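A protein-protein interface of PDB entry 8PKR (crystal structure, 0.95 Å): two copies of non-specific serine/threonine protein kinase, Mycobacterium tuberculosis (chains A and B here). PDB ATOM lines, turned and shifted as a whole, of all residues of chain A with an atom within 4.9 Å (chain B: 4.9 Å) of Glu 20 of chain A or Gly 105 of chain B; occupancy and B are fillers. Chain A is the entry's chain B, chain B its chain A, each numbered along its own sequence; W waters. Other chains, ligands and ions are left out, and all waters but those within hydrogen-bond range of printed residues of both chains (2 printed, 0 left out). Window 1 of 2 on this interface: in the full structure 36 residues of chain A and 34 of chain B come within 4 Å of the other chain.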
ATOM      1  N   TYR A  18     -17.126  15.862  -5.265  1.00  0.00           N
ATOM      2  CA  TYR A  18     -15.955  16.358  -5.987  1.00  0.00           C
ATOM      3  C   TYR A  18     -15.619  15.418  -7.145  1.00  0.00           C
ATOM      4  O   TYR A  18     -14.477  14.964  -7.301  1.00  0.00           O
ATOM      5  CB  TYR A  18     -14.785  16.542  -5.006  1.00  0.00           C
ATOM      6  CG  TYR A  18     -13.768  17.581  -5.346  1.00  0.00           C
ATOM      7  CD1 TYR A  18     -14.029  18.922  -5.196  1.00  0.00           C
ATOM      8  CD2 TYR A  18     -12.510  17.204  -5.786  1.00  0.00           C
ATOM      9  CE1 TYR A  18     -13.061  19.872  -5.484  1.00  0.00           C
ATOM     10  CE2 TYR A  18     -11.551  18.127  -6.080  1.00  0.00           C
ATOM     11  CZ  TYR A  18     -11.829  19.462  -5.926  1.00  0.00           C
ATOM     12  OH  TYR A  18     -10.867  20.393  -6.224  1.00  0.00           O
ATOM     13  N   PRO A  19     -16.594  15.124  -8.002  1.00  0.00           N
ATOM     14  CA  PRO A  19     -16.319  14.265  -9.154  1.00  0.00           C
ATOM     15  C   PRO A  19     -15.253  14.906 -10.039  1.00  0.00           C
ATOM     16  O   PRO A  19     -15.232  16.121 -10.232  1.00  0.00           O
ATOM     17  CB  PRO A  19     -17.675  14.182  -9.864  1.00  0.00           C
ATOM     18  CG  PRO A  19     -18.349  15.482  -9.494  1.00  0.00           C
ATOM     19  CD  PRO A  19     -17.950  15.703  -8.070  1.00  0.00           C
ATOM     20  N   GLU A  20     -14.374  14.067 -10.578  1.00  0.00           N
ATOM     21  CA  GLU A  20     -13.203  14.514 -11.334  1.00  0.00           C
ATOM     22  C   GLU A  20     -13.392  14.157 -12.802  1.00  0.00           C
ATOM     23  O   GLU A  20     -14.280  14.704 -13.459  1.00  0.00           O
ATOM     24  CB  GLU A  20     -11.938  13.962 -10.668  1.00  0.00           C
ATOM     25  CG  GLU A  20     -11.629  14.574  -9.314  1.00  0.00           C
ATOM     26  CD  GLU A  20     -10.718  15.827  -9.352  1.00  0.00           C
ATOM     27  OE1 GLU A  20     -10.116  16.140 -10.394  1.00  0.00           O
ATOM     28  OE2 GLU A  20     -10.538  16.396  -8.256  1.00  0.00           O
ATOM     29  N   GLY A  21     -12.587  13.250 -13.343  1.00  0.00           N
ATOM     30  CA  GLY A  21     -12.772  12.840 -14.714  1.00  0.00           C
ATOM     31  C   GLY A  21     -14.019  11.994 -14.907  1.00  0.00           C
ATOM     32  O   GLY A  21     -14.559  11.392 -13.972  1.00  0.00           O
ATOM     33  N   LEU A  22     -14.456  11.940 -16.160  1.00  0.00           N
ATOM     34  CA  LEU A  22     -15.540  11.062 -16.574  1.00  0.00           C
ATOM     35  C   LEU A  22     -15.227  10.510 -17.963  1.00  0.00           C
ATOM     36  O   LEU A  22     -14.364  11.026 -18.692  1.00  0.00           O
ATOM     37  CB  LEU A  22     -16.927  11.738 -16.503  1.00  0.00           C
ATOM     38  CG  LEU A  22     -17.339  12.708 -17.600  1.00  0.00           C
ATOM     39  CD1 LEU A  22     -18.766  13.175 -17.353  1.00  0.00           C
ATOM     40  CD2 LEU A  22     -16.401  13.909 -17.716  1.00  0.00           C
ATOM     41  N   VAL A  32     -17.760   7.870 -13.875  1.00  0.00           N
ATOM     42  CA  VAL A  32     -17.267   9.032 -13.149  1.00  0.00           C
ATOM     43  C   VAL A  32     -16.280   8.602 -12.079  1.00  0.00           C
ATOM     44  O   VAL A  32     -16.568   7.696 -11.290  1.00  0.00           O
ATOM     45  CB  VAL A  32     -18.417   9.823 -12.504  1.00  0.00           C
ATOM     46  CG1 VAL A  32     -17.895  10.983 -11.671  1.00  0.00           C
ATOM     47  CG2 VAL A  32     -19.395  10.305 -13.547  1.00  0.00           C
ATOM     48  N   ALA A  33     -15.129   9.284 -12.040  1.00  0.00           N
ATOM     49  CA  ALA A  33     -14.180   9.151 -10.935  1.00  0.00           C
ATOM     50  C   ALA A  33     -14.687  10.023  -9.794  1.00  0.00           C
ATOM     51  O   ALA A  33     -14.506  11.244  -9.785  1.00  0.00           O
ATOM     52  CB  ALA A  33     -12.786   9.578 -11.385  1.00  0.00           C
ATOM     53  N   ARG A  35     -14.142  11.171  -6.709  1.00  0.00           N
ATOM     54  CA  ARG A  35     -12.945  11.263  -5.883  1.00  0.00           C
ATOM     55  C   ARG A  35     -13.273  11.236  -4.398  1.00  0.00           C
ATOM     56  O   ARG A  35     -12.623  10.530  -3.615  1.00  0.00           O
ATOM     57  CB  ARG A  35     -12.196  12.569  -6.227  1.00  0.00           C
ATOM     58  CG  ARG A  35     -10.982  12.833  -5.370  1.00  0.00           C
ATOM     59  CD  ARG A  35     -10.455  14.257  -5.586  1.00  0.00           C
ATOM     60  NE  ARG A  35      -9.544  14.705  -4.548  1.00  0.00           N
ATOM     61  CZ  ARG A  35      -8.219  14.600  -4.589  1.00  0.00           C
ATOM     62  NH1 ARG A  35      -7.610  14.084  -5.644  1.00  0.00           N
ATOM     63  NH2 ARG A  35      -7.512  15.008  -3.549  1.00  0.00           N
ATOM     64  N   PRO A  61      -9.555   8.638  -6.485  1.00  0.00           N
ATOM     65  CA  PRO A  61      -9.533   8.406  -7.930  1.00  0.00           C
ATOM     66  C   PRO A  61      -9.840   9.706  -8.671  1.00  0.00           C
ATOM     67  O   PRO A  61     -10.806  10.401  -8.358  1.00  0.00           O
ATOM     68  CB  PRO A  61     -10.639   7.368  -8.130  1.00  0.00           C
ATOM     69  CG  PRO A  61     -11.612   7.642  -6.994  1.00  0.00           C
ATOM     70  CD  PRO A  61     -10.704   7.979  -5.834  1.00  0.00           C
ATOM     71  N   ASP A  62      -9.022  10.019  -9.687  1.00  0.00           N
ATOM     72  CA  ASP A  62      -9.142  11.309 -10.360  1.00  0.00           C
ATOM     73  C   ASP A  62      -9.502  11.222 -11.833  1.00  0.00           C
ATOM     74  O   ASP A  62      -9.931  12.234 -12.395  1.00  0.00           O
ATOM     75  CB  ASP A  62      -7.875  12.152 -10.177  1.00  0.00           C
ATOM     76  CG  ASP A  62      -7.792  12.690  -8.752  1.00  0.00           C
ATOM     77  OD1 ASP A  62      -8.782  13.264  -8.256  1.00  0.00           O
ATOM     78  OD2 ASP A  62      -6.753  12.482  -8.077  1.00  0.00           O
ATOM     79  N   TRP A 104      -2.966  11.205 -12.586  1.00  0.00           N
ATOM     80  CA  TRP A 104      -4.076  12.135 -12.416  1.00  0.00           C
ATOM     81  C   TRP A 104      -5.101  11.961 -13.539  1.00  0.00           C
ATOM     82  O   TRP A 104      -6.132  11.301 -13.363  1.00  0.00           O
ATOM     83  CB  TRP A 104      -3.542  13.589 -12.298  1.00  0.00           C
ATOM     84  CG  TRP A 104      -4.618  14.496 -11.865  1.00  0.00           C
ATOM     85  CD1 TRP A 104      -5.542  15.103 -12.658  1.00  0.00           C
ATOM     86  CD2 TRP A 104      -4.937  14.854 -10.529  1.00  0.00           C
ATOM     87  NE1 TRP A 104      -6.448  15.786 -11.895  1.00  0.00           N
ATOM     88  CE2 TRP A 104      -6.080  15.679 -10.581  1.00  0.00           C
ATOM     89  CE3 TRP A 104      -4.355  14.585  -9.298  1.00  0.00           C
ATOM     90  CZ2 TRP A 104      -6.641  16.246  -9.434  1.00  0.00           C
ATOM     91  CZ3 TRP A 104      -4.911  15.144  -8.163  1.00  0.00           C
ATOM     92  CH2 TRP A 104      -6.052  15.953  -8.236  1.00  0.00           C
ATOM     93  N   ASP B  62      -9.288  22.520 -17.217  1.00  0.00           N
ATOM     94  CA  ASP B  62      -9.086  21.266 -16.507  1.00  0.00           C
ATOM     95  C   ASP B  62      -9.179  20.018 -17.368  1.00  0.00           C
ATOM     96  O   ASP B  62      -8.484  19.041 -17.085  1.00  0.00           O
ATOM     97  CB  ASP B  62     -10.049  21.135 -15.328  1.00  0.00           C
ATOM     98  CG  ASP B  62      -9.422  20.368 -14.237  1.00  0.00           C
ATOM     99  OD1 ASP B  62      -8.604  21.006 -13.520  1.00  0.00           O
ATOM    100  OD2 ASP B  62      -9.666  19.140 -14.166  1.00  0.00           O
ATOM    101  N   THR B  75     -12.890  22.155 -20.923  1.00  0.00           N
ATOM    102  CA  THR B  75     -13.546  22.782 -19.785  1.00  0.00           C
ATOM    103  C   THR B  75     -12.682  23.936 -19.294  1.00  0.00           C
ATOM    104  O   THR B  75     -11.592  23.742 -18.745  1.00  0.00           O
ATOM    105  CB  THR B  75     -13.829  21.768 -18.674  1.00  0.00           C
ATOM    106  OG1 THR B  75     -12.623  21.045 -18.443  1.00  0.00           O
ATOM    107  CG2 THR B  75     -14.967  20.837 -19.044  1.00  0.00           C
ATOM    108  N   PRO B 103     -17.126  23.840 -14.549  1.00  0.00           N
ATOM    109  CA  PRO B 103     -17.030  22.582 -15.304  1.00  0.00           C
ATOM    110  C   PRO B 103     -15.600  22.063 -15.237  1.00  0.00           C
ATOM    111  O   PRO B 103     -14.643  22.841 -15.286  1.00  0.00           O
ATOM    112  CB  PRO B 103     -17.406  22.996 -16.728  1.00  0.00           C
ATOM    113  CG  PRO B 103     -16.924  24.438 -16.829  1.00  0.00           C
ATOM    114  CD  PRO B 103     -17.217  25.008 -15.446  1.00  0.00           C
ATOM    115  N   TRP B 104     -15.459  20.746 -15.129  1.00  0.00           N
ATOM    116  CA  TRP B 104     -14.208  20.155 -14.656  1.00  0.00           C
ATOM    117  C   TRP B 104     -13.744  19.046 -15.599  1.00  0.00           C
ATOM    118  O   TRP B 104     -12.919  19.279 -16.489  1.00  0.00           O
ATOM    119  CB  TRP B 104     -14.403  19.697 -13.214  1.00  0.00           C
ATOM    120  CG  TRP B 104     -13.167  19.337 -12.554  1.00  0.00           C
ATOM    121  CD1 TRP B 104     -12.602  18.102 -12.496  1.00  0.00           C
ATOM    122  CD2 TRP B 104     -12.297  20.216 -11.845  1.00  0.00           C
ATOM    123  NE1 TRP B 104     -11.452  18.144 -11.768  1.00  0.00           N
ATOM    124  CE2 TRP B 104     -11.234  19.433 -11.358  1.00  0.00           C
ATOM    125  CE3 TRP B 104     -12.349  21.558 -11.514  1.00  0.00           C
ATOM    126  CZ2 TRP B 104     -10.213  19.968 -10.583  1.00  0.00           C
ATOM    127  CZ3 TRP B 104     -11.340  22.086 -10.747  1.00  0.00           C
ATOM    128  CH2 TRP B 104     -10.278  21.305 -10.308  1.00  0.00           C
ATOM    129  N   GLY B 105     -14.269  17.831 -15.446  1.00  0.00           N
ATOM    130  CA  GLY B 105     -13.961  16.780 -16.382  1.00  0.00           C
ATOM    131  C   GLY B 105     -14.823  16.876 -17.627  1.00  0.00           C
ATOM    132  O   GLY B 105     -15.926  17.428 -17.588  1.00  0.00           O
ATOM    133  N   ILE B 106     -14.320  16.313 -18.734  1.00  0.00           N
ATOM    134  CA  ILE B 106     -15.080  16.293 -19.976  1.00  0.00           C
ATOM    135  C   ILE B 106     -14.871  14.980 -20.705  1.00  0.00           C
ATOM    136  O   ILE B 106     -13.782  14.389 -20.678  1.00  0.00           O
ATOM    137  CB  ILE B 106     -14.700  17.487 -20.887  1.00  0.00           C
ATOM    138  CG1 ILE B 106     -15.615  17.616 -22.091  1.00  0.00           C
ATOM    139  CG2 ILE B 106     -13.221  17.450 -21.298  1.00  0.00           C
ATOM    140  CD1 ILE B 106     -15.547  19.009 -22.718  1.00  0.00           C
ATOM    141  N   ALA B 107     -15.917  14.559 -21.410  1.00  0.00           N
ATOM    142  CA  ALA B 107     -15.853  13.456 -22.358  1.00  0.00           C
ATOM    143  C   ALA B 107     -16.833  13.748 -23.481  1.00  0.00           C
ATOM    144  O   ALA B 107     -17.846  14.413 -23.269  1.00  0.00           O
ATOM    145  CB  ALA B 107     -16.203  12.118 -21.689  1.00  0.00           C
ATOM    146  N   TYR B 115     -20.245  15.655 -22.258  1.00  0.00           N
ATOM    147  CA  TYR B 115     -20.560  15.357 -20.874  1.00  0.00           C
ATOM    148  C   TYR B 115     -19.496  16.001 -20.002  1.00  0.00           C
ATOM    149  O   TYR B 115     -18.303  15.847 -20.291  1.00  0.00           O
ATOM    150  CB  TYR B 115     -20.531  13.842 -20.623  1.00  0.00           C
ATOM    151  CG  TYR B 115     -21.411  13.022 -21.535  1.00  0.00           C
ATOM    152  CD1 TYR B 115     -21.029  12.733 -22.833  1.00  0.00           C
ATOM    153  CD2 TYR B 115     -22.634  12.521 -21.093  1.00  0.00           C
ATOM    154  CE1 TYR B 115     -21.815  11.967 -23.656  1.00  0.00           C
ATOM    155  CE2 TYR B 115     -23.431  11.736 -21.919  1.00  0.00           C
ATOM    156  CZ  TYR B 115     -23.021  11.457 -23.200  1.00  0.00           C
ATOM    157  OH  TYR B 115     -23.832  10.680 -24.003  1.00  0.00           O
ATOM    158  N   VAL B 116     -19.911  16.686 -18.940  1.00  0.00           N
ATOM    159  CA  VAL B 116     -18.959  17.295 -18.022  1.00  0.00           C
ATOM    160  C   VAL B 116     -19.330  16.981 -16.584  1.00  0.00           C
ATOM    161  O   VAL B 116     -20.510  16.833 -16.245  1.00  0.00           O
ATOM    162  CB  VAL B 116     -18.830  18.832 -18.199  1.00  0.00           C
ATOM    163  CG1 VAL B 116     -18.308  19.152 -19.583  1.00  0.00           C
ATOM    164  CG2 VAL B 116     -20.137  19.564 -17.931  1.00  0.00           C
ATOM    165  N   THR B 117     -18.316  16.895 -15.721  1.00  0.00           N
ATOM    166  CA  THR B 117     -18.545  17.032 -14.295  1.00  0.00           C
ATOM    167  C   THR B 117     -18.425  18.508 -13.927  1.00  0.00           C
ATOM    168  O   THR B 117     -17.783  19.282 -14.641  1.00  0.00           O
ATOM    169  CB  THR B 117     -17.566  16.202 -13.474  1.00  0.00           C
ATOM    170  OG1 THR B 117     -16.237  16.620 -13.802  1.00  0.00           O
ATOM    171  CG2 THR B 117     -17.716  14.720 -13.730  1.00  0.00           C
ATOM    172  N   HIS B 119     -17.975  21.229 -10.392  1.00  0.00           N
ATOM    173  CA  HIS B 119     -17.613  21.256  -8.988  1.00  0.00           C
ATOM    174  C   HIS B 119     -18.459  22.191  -8.142  1.00  0.00           C
ATOM    175  O   HIS B 119     -18.296  22.211  -6.914  1.00  0.00           O
ATOM    176  CB  HIS B 119     -16.146  21.598  -8.826  1.00  0.00           C
ATOM    177  CG  HIS B 119     -15.256  20.415  -9.017  1.00  0.00           C
ATOM    178  ND1 HIS B 119     -13.914  20.467  -8.730  1.00  0.00           N
ATOM    179  CD2 HIS B 119     -15.500  19.152  -9.442  1.00  0.00           C
ATOM    180  CE1 HIS B 119     -13.368  19.294  -8.964  1.00  0.00           C
ATOM    181  NE2 HIS B 119     -14.307  18.478  -9.392  1.00  0.00           N
HETATM  182  O   HOH W   1     -12.823  22.761  -7.655  1.00  0.00           O
HETATM  183  O   HOH W   2     -12.574  13.152 -18.103  1.00  0.00           O
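The backbone carbonyl oxygen of Glu 20 of chain A is in hydrogen-bond range of the side-chain hydroxyl of Thr 117 of chain B.
OE1 of Glu 20 of chain A lies within hydrogen-bond range of NE1 of Trp 104 of chain B, at 2.8 Å.
O of Pro 19 of chain A lies within hydrogen-bond range of NE2 of His 119 of chain B (2.7 Å).
2 positions are printed for both chains.
Of the 12 pairs that touch across the chains among the printed residues, none has its exchanged pair printed and touching as well.
Tyr 18 of chain A touches His 119 of chain B (CE1 to ND1, 3.4 Å).
CD1 of Trp 104 of chain B touches O of Pro 19 of chain A (3.996 Å).
OG1 of Thr 117 of chain B touches O of Pro 19 of chain A, 3.7 Å away.
Glu 20 of chain A touches Gly 105 of chain B (O to CA, 3.6 Å).
Gly 105 of chain B touches Leu 22 of chain A (C to CD2, 3.4 Å).
N of Ile 106 of chain B touches CD2 of Leu 22 of chain A, at 3.3 Å.
O of Leu 22 of chain A touches CB of Ala 107 of chain B, at 3.7 Å.
CD2 of Leu 22 of chain A touches O of Tyr 115 of chain B (3.7 Å).
CD1 of Leu 22 of chain A touches C of Val 116 of chain B (3.9 Å).
The backbone carbonyl oxygen (O) of Thr 117 of chain B lies within hydrogen-bond range of the backbone NH (N) of Trp 104 of chain B.
N of Glu 20 of chain A lies within hydrogen-bond range of O of Ala 33 of chain A.
N of Gly 105 of chain B is in hydrogen-bond range of OG1 of Thr 117 of chain B.
The side-chain hydroxyl (OG1) of Thr 75 of chain B is in hydrogen-bond range of the backbone carbonyl oxygen (O) of Trp 104 of chain B (2.7 Å).
The side-chain carboxylate (OD2) of Asp 62 of chain B sits at hydrogen-bond distance from the indole nitrogen (NE1) of Trp 104 of chain B (3.2 Å).
The backbone carbonyl oxygen of Ala 107 of chain B sits at hydrogen-bond distance from the backbone NH of Tyr 115 of chain B (2.9 Å).
Hydrophobic or aromatic side chains of chain A within 4 Å of the printed part of chain B: Tyr 18, Pro 19 and Leu 22.
Among the printed residues, 12 pairs touch across the chains.
Water W1 bridges ND1 of His 119 of chain B (2.8 Å) and OH of Tyr 18 of chain A (3.4 Å).
Water W2 lies within hydrogen-bond range of O of Leu 22 of chain A (2.8 Å) and O of Ile 106 of chain B (3.1 Å).
Of chain B, only Trp 104, Gly 105 and Thr 117 come within 4 Å of Glu 20 of chain A.
Of chain A, only Glu 20 (3.6 Å) and Leu 22 (3.4 Å) come within 4 Å of Gly 105 of chain B.
Printed residues of chain A within 4 Å of Thr 117 of chain B: Pro 19 and Glu 20.
Of the printed residues of chain A, His 119 of chain B touches Tyr 18 (3.4 Å) and Pro 19 (2.7 Å).
The nearest printed residue of chain A that does not touch His 119 of chain B is Glu 20 of chain A (4.1 Å).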
